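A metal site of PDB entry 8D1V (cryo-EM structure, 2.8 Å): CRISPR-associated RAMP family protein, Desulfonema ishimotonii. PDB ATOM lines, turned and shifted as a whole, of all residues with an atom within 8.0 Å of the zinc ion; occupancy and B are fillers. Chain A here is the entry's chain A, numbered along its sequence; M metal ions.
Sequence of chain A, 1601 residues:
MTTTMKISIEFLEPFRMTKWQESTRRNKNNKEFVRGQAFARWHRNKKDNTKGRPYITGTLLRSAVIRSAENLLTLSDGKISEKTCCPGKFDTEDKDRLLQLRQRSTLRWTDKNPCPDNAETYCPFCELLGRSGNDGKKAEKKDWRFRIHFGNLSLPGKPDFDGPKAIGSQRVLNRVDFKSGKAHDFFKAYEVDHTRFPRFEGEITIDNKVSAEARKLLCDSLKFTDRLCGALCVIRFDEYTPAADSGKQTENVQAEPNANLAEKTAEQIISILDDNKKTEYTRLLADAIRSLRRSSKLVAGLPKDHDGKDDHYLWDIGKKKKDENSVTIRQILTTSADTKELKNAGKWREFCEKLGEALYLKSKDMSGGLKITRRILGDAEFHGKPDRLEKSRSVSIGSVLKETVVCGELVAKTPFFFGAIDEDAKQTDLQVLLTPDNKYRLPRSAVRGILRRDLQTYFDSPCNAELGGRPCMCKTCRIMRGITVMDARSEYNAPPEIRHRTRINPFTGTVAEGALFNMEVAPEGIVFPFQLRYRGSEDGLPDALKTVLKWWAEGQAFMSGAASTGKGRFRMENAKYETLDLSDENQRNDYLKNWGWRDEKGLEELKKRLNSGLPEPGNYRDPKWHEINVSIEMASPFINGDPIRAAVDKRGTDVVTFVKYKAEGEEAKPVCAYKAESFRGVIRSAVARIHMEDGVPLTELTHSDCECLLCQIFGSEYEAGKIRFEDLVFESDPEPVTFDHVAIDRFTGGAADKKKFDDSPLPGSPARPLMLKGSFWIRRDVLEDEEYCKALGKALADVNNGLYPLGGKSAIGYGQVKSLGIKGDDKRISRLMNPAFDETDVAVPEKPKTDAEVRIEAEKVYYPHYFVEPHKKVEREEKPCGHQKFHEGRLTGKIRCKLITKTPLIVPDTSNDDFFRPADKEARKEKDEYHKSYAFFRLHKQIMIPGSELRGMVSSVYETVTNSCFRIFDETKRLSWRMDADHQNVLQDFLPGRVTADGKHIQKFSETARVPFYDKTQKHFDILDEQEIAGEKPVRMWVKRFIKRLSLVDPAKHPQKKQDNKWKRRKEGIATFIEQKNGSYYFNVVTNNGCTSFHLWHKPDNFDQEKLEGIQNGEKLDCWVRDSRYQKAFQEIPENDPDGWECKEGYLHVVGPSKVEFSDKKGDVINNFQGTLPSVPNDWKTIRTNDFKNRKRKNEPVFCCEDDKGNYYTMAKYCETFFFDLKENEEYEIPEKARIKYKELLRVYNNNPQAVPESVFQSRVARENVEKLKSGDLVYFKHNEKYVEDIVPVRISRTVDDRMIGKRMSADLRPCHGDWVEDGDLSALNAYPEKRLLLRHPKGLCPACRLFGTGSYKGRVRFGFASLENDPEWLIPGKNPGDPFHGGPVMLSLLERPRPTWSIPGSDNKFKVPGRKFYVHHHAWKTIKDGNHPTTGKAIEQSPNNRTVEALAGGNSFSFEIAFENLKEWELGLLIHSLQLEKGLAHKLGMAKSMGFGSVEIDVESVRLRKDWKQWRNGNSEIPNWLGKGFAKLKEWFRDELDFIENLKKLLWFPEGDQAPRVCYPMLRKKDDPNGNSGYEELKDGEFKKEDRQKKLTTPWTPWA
Four residues have an atom within 4 Å of the zinc ion: Cys 463, Cys 472, Cys 474 and Cys 477.
The nearest printed residue that does not touch the zinc ion is Ala 465 (4.3 Å).
The zinc ion is bound by SG of Cys 477, SG of Cys 463, SG of Cys 474 and SG of Cys 472.
N of Ala 465 sits close to SG of Cys 463 (3.7 Å).
OE1 of Gln 456 sits at hydrogen-bond distance from N of Cys 463.
The backbone NH of Thr 476 sits close to the side-chain sulfur of Cys 474 (3.6 Å).
O of Cys 472 is in hydrogen-bond range of NH1 of Arg 481 (2.6 Å).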
ATOM      1  N   ARG A 452     -28.681  -2.936  -6.912  1.00  0.00           N
ATOM      2  CA  ARG A 452     -28.368  -4.171  -6.212  1.00  0.00           C
ATOM      3  C   ARG A 452     -29.140  -5.345  -6.787  1.00  0.00           C
ATOM      4  O   ARG A 452     -28.604  -6.453  -6.940  1.00  0.00           O
ATOM      5  CB  ARG A 452     -28.649  -4.021  -4.717  1.00  0.00           C
ATOM      6  CG  ARG A 452     -28.653  -5.333  -3.964  1.00  0.00           C
ATOM      7  CD  ARG A 452     -28.919  -5.127  -2.491  1.00  0.00           C
ATOM      8  NE  ARG A 452     -28.036  -4.115  -1.920  1.00  0.00           N
ATOM      9  CZ  ARG A 452     -26.753  -4.300  -1.650  1.00  0.00           C
ATOM     10  NH1 ARG A 452     -26.148  -5.445  -1.915  1.00  0.00           N
ATOM     11  NH2 ARG A 452     -26.055  -3.310  -1.110  1.00  0.00           N
ATOM     12  N   GLN A 456     -27.394  -8.554  -9.008  1.00  0.00           N
ATOM     13  CA  GLN A 456     -27.592  -9.963  -8.699  1.00  0.00           C
ATOM     14  C   GLN A 456     -28.070 -10.744  -9.915  1.00  0.00           C
ATOM     15  O   GLN A 456     -27.667 -11.896 -10.114  1.00  0.00           O
ATOM     16  CB  GLN A 456     -28.584 -10.106  -7.542  1.00  0.00           C
ATOM     17  CG  GLN A 456     -27.964  -9.863  -6.191  1.00  0.00           C
ATOM     18  CD  GLN A 456     -28.979  -9.428  -5.161  1.00  0.00           C
ATOM     19  OE1 GLN A 456     -29.341 -10.184  -4.270  1.00  0.00           O
ATOM     20  NE2 GLN A 456     -29.441  -8.189  -5.278  1.00  0.00           N
ATOM     21  N   SER A 461     -26.401 -14.886  -9.050  1.00  0.00           N
ATOM     22  CA  SER A 461     -26.241 -15.288  -7.675  1.00  0.00           C
ATOM     23  C   SER A 461     -26.894 -14.262  -6.765  1.00  0.00           C
ATOM     24  O   SER A 461     -26.469 -13.098  -6.754  1.00  0.00           O
ATOM     25  CB  SER A 461     -24.752 -15.419  -7.313  1.00  0.00           C
ATOM     26  OG  SER A 461     -24.091 -16.365  -8.150  1.00  0.00           O
ATOM     27  N   PRO A 462     -27.925 -14.627  -6.015  1.00  0.00           N
ATOM     28  CA  PRO A 462     -28.472 -13.707  -5.022  1.00  0.00           C
ATOM     29  C   PRO A 462     -27.495 -13.502  -3.877  1.00  0.00           C
ATOM     30  O   PRO A 462     -26.540 -14.252  -3.686  1.00  0.00           O
ATOM     31  CB  PRO A 462     -29.756 -14.394  -4.551  1.00  0.00           C
ATOM     32  CG  PRO A 462     -30.022 -15.485  -5.559  1.00  0.00           C
ATOM     33  CD  PRO A 462     -28.681 -15.881  -6.089  1.00  0.00           C
ATOM     34  N   CYS A 463     -27.733 -12.437  -3.112  1.00  0.00           N
ATOM     35  CA  CYS A 463     -26.978 -12.138  -1.913  1.00  0.00           C
ATOM     36  C   CYS A 463     -27.841 -12.480  -0.706  1.00  0.00           C
ATOM     37  O   CYS A 463     -28.910 -11.895  -0.503  1.00  0.00           O
ATOM     38  CB  CYS A 463     -26.554 -10.673  -1.875  1.00  0.00           C
ATOM     39  SG  CYS A 463     -25.771 -10.216  -0.316  1.00  0.00           S
ATOM     40  N   ASN A 464     -27.389 -13.443   0.087  1.00  0.00           N
ATOM     41  CA  ASN A 464     -28.142 -13.940   1.238  1.00  0.00           C
ATOM     42  C   ASN A 464     -27.639 -13.378   2.559  1.00  0.00           C
ATOM     43  O   ASN A 464     -28.059 -13.861   3.620  1.00  0.00           O
ATOM     44  CB  ASN A 464     -28.128 -15.466   1.252  1.00  0.00           C
ATOM     45  CG  ASN A 464     -26.735 -16.063   1.422  1.00  0.00           C
ATOM     46  OD1 ASN A 464     -25.762 -15.354   1.653  1.00  0.00           O
ATOM     47  ND2 ASN A 464     -26.653 -17.380   1.312  1.00  0.00           N
ATOM     48  N   ALA A 465     -26.762 -12.382   2.537  1.00  0.00           N
ATOM     49  CA  ALA A 465     -26.246 -11.804   3.767  1.00  0.00           C
ATOM     50  C   ALA A 465     -27.348 -11.090   4.539  1.00  0.00           C
ATOM     51  O   ALA A 465     -28.233 -10.443   3.953  1.00  0.00           O
ATOM     52  CB  ALA A 465     -25.112 -10.822   3.465  1.00  0.00           C
ATOM     53  N   GLU A 466     -27.300 -11.208   5.856  1.00  0.00           N
ATOM     54  CA  GLU A 466     -28.264 -10.559   6.724  1.00  0.00           C
ATOM     55  C   GLU A 466     -27.711  -9.229   7.227  1.00  0.00           C
ATOM     56  O   GLU A 466     -26.535  -8.907   7.067  1.00  0.00           O
ATOM     57  CB  GLU A 466     -28.651 -11.482   7.881  1.00  0.00           C
ATOM     58  CG  GLU A 466     -27.523 -11.756   8.868  1.00  0.00           C
ATOM     59  CD  GLU A 466     -26.748 -13.015   8.524  1.00  0.00           C
ATOM     60  OE1 GLU A 466     -27.080 -13.665   7.524  1.00  0.00           O
ATOM     61  OE2 GLU A 466     -25.793 -13.346   9.261  1.00  0.00           O
ATOM     62  N   PRO A 471     -19.043  -6.722   6.738  1.00  0.00           N
ATOM     63  CA  PRO A 471     -19.644  -6.529   5.411  1.00  0.00           C
ATOM     64  C   PRO A 471     -19.569  -7.786   4.551  1.00  0.00           C
ATOM     65  O   PRO A 471     -18.556  -8.488   4.535  1.00  0.00           O
ATOM     66  CB  PRO A 471     -18.809  -5.390   4.797  1.00  0.00           C
ATOM     67  CG  PRO A 471     -18.240  -4.685   5.964  1.00  0.00           C
ATOM     68  CD  PRO A 471     -18.026  -5.704   7.031  1.00  0.00           C
ATOM     69  N   CYS A 472     -20.654  -8.049   3.832  1.00  0.00           N
ATOM     70  CA  CYS A 472     -20.689  -9.175   2.916  1.00  0.00           C
ATOM     71  C   CYS A 472     -19.658  -8.998   1.813  1.00  0.00           C
ATOM     72  O   CYS A 472     -19.494  -7.901   1.282  1.00  0.00           O
ATOM     73  CB  CYS A 472     -22.091  -9.323   2.318  1.00  0.00           C
ATOM     74  SG  CYS A 472     -22.373 -10.856   1.395  1.00  0.00           S
ATOM     75  N   MET A 473     -18.960 -10.073   1.482  1.00  0.00           N
ATOM     76  CA  MET A 473     -17.861 -10.023   0.520  1.00  0.00           C
ATOM     77  C   MET A 473     -18.227 -10.653  -0.815  1.00  0.00           C
ATOM     78  O   MET A 473     -17.350 -11.018  -1.599  1.00  0.00           O
ATOM     79  CB  MET A 473     -16.619 -10.692   1.111  1.00  0.00           C
ATOM     80  CG  MET A 473     -16.150 -10.099   2.417  1.00  0.00           C
ATOM     81  SD  MET A 473     -15.647  -8.369   2.299  1.00  0.00           S
ATOM     82  CE  MET A 473     -14.572  -8.439   0.870  1.00  0.00           C
ATOM     83  N   CYS A 474     -19.516 -10.779  -1.110  1.00  0.00           N
ATOM     84  CA  CYS A 474     -19.957 -11.291  -2.397  1.00  0.00           C
ATOM     85  C   CYS A 474     -19.738 -10.234  -3.463  1.00  0.00           C
ATOM     86  O   CYS A 474     -19.452  -9.069  -3.159  1.00  0.00           O
ATOM     87  CB  CYS A 474     -21.432 -11.711  -2.359  1.00  0.00           C
ATOM     88  SG  CYS A 474     -22.626 -10.376  -2.460  1.00  0.00           S
ATOM     89  N   LYS A 475     -19.842 -10.650  -4.722  1.00  0.00           N
ATOM     90  CA  LYS A 475     -19.527  -9.761  -5.829  1.00  0.00           C
ATOM     91  C   LYS A 475     -20.473  -8.558  -5.858  1.00  0.00           C
ATOM     92  O   LYS A 475     -20.058  -7.454  -6.235  1.00  0.00           O
ATOM     93  CB  LYS A 475     -19.583 -10.518  -7.152  1.00  0.00           C
ATOM     94  CG  LYS A 475     -18.633 -11.693  -7.232  1.00  0.00           C
ATOM     95  CD  LYS A 475     -19.029 -12.659  -8.320  1.00  0.00           C
ATOM     96  CE  LYS A 475     -20.377 -13.315  -8.016  1.00  0.00           C
ATOM     97  NZ  LYS A 475     -20.766 -14.288  -9.064  1.00  0.00           N
ATOM     98  N   THR A 476     -21.737  -8.768  -5.502  1.00  0.00           N
ATOM     99  CA  THR A 476     -22.706  -7.680  -5.524  1.00  0.00           C
ATOM    100  C   THR A 476     -22.430  -6.675  -4.421  1.00  0.00           C
ATOM    101  O   THR A 476     -22.405  -5.464  -4.668  1.00  0.00           O
ATOM    102  CB  THR A 476     -24.126  -8.240  -5.407  1.00  0.00           C
ATOM    103  OG1 THR A 476     -24.454  -8.950  -6.603  1.00  0.00           O
ATOM    104  CG2 THR A 476     -25.129  -7.123  -5.189  1.00  0.00           C
ATOM    105  N   CYS A 477     -22.201  -7.148  -3.195  1.00  0.00           N
ATOM    106  CA  CYS A 477     -21.919  -6.236  -2.085  1.00  0.00           C
ATOM    107  C   CYS A 477     -20.626  -5.468  -2.297  1.00  0.00           C
ATOM    108  O   CYS A 477     -20.547  -4.303  -1.913  1.00  0.00           O
ATOM    109  CB  CYS A 477     -21.849  -6.992  -0.768  1.00  0.00           C
ATOM    110  SG  CYS A 477     -23.436  -7.511  -0.122  1.00  0.00           S
ATOM    111  N   ARG A 478     -19.606  -6.099  -2.868  1.00  0.00           N
ATOM    112  CA  ARG A 478     -18.342  -5.412  -3.099  1.00  0.00           C
ATOM    113  C   ARG A 478     -18.511  -4.245  -4.057  1.00  0.00           C
ATOM    114  O   ARG A 478     -17.951  -3.169  -3.864  1.00  0.00           O
ATOM    115  CB  ARG A 478     -17.298  -6.396  -3.615  1.00  0.00           C
ATOM    116  CG  ARG A 478     -16.684  -7.260  -2.529  1.00  0.00           C
ATOM    117  CD  ARG A 478     -15.453  -7.996  -3.031  1.00  0.00           C
ATOM    118  NE  ARG A 478     -15.703  -9.418  -3.239  1.00  0.00           N
ATOM    119  CZ  ARG A 478     -15.795  -9.997  -4.425  1.00  0.00           C
ATOM    120  NH1 ARG A 478     -15.652  -9.304  -5.546  1.00  0.00           N
ATOM    121  NH2 ARG A 478     -16.026 -11.307  -4.495  1.00  0.00           N
ATOM    122  N   ARG A 481     -20.535  -1.297  -2.383  1.00  0.00           N
ATOM    123  CA  ARG A 481     -19.852  -0.495  -1.376  1.00  0.00           C
ATOM    124  C   ARG A 481     -18.995   0.603  -1.981  1.00  0.00           C
ATOM    125  O   ARG A 481     -18.540   1.490  -1.248  1.00  0.00           O
ATOM    126  CB  ARG A 481     -18.988  -1.396  -0.493  1.00  0.00           C
ATOM    127  CG  ARG A 481     -19.769  -2.070   0.604  1.00  0.00           C
ATOM    128  CD  ARG A 481     -18.859  -2.573   1.691  1.00  0.00           C
ATOM    129  NE  ARG A 481     -17.865  -3.488   1.162  1.00  0.00           N
ATOM    130  CZ  ARG A 481     -18.031  -4.798   1.063  1.00  0.00           C
ATOM    131  NH1 ARG A 481     -19.145  -5.381   1.482  1.00  0.00           N
ATOM    132  NH2 ARG A 481     -17.059  -5.544   0.543  1.00  0.00           N
HETATM  133 ZN    ZN M   1     -23.489  -9.814  -0.371  1.00  0.00          ZN
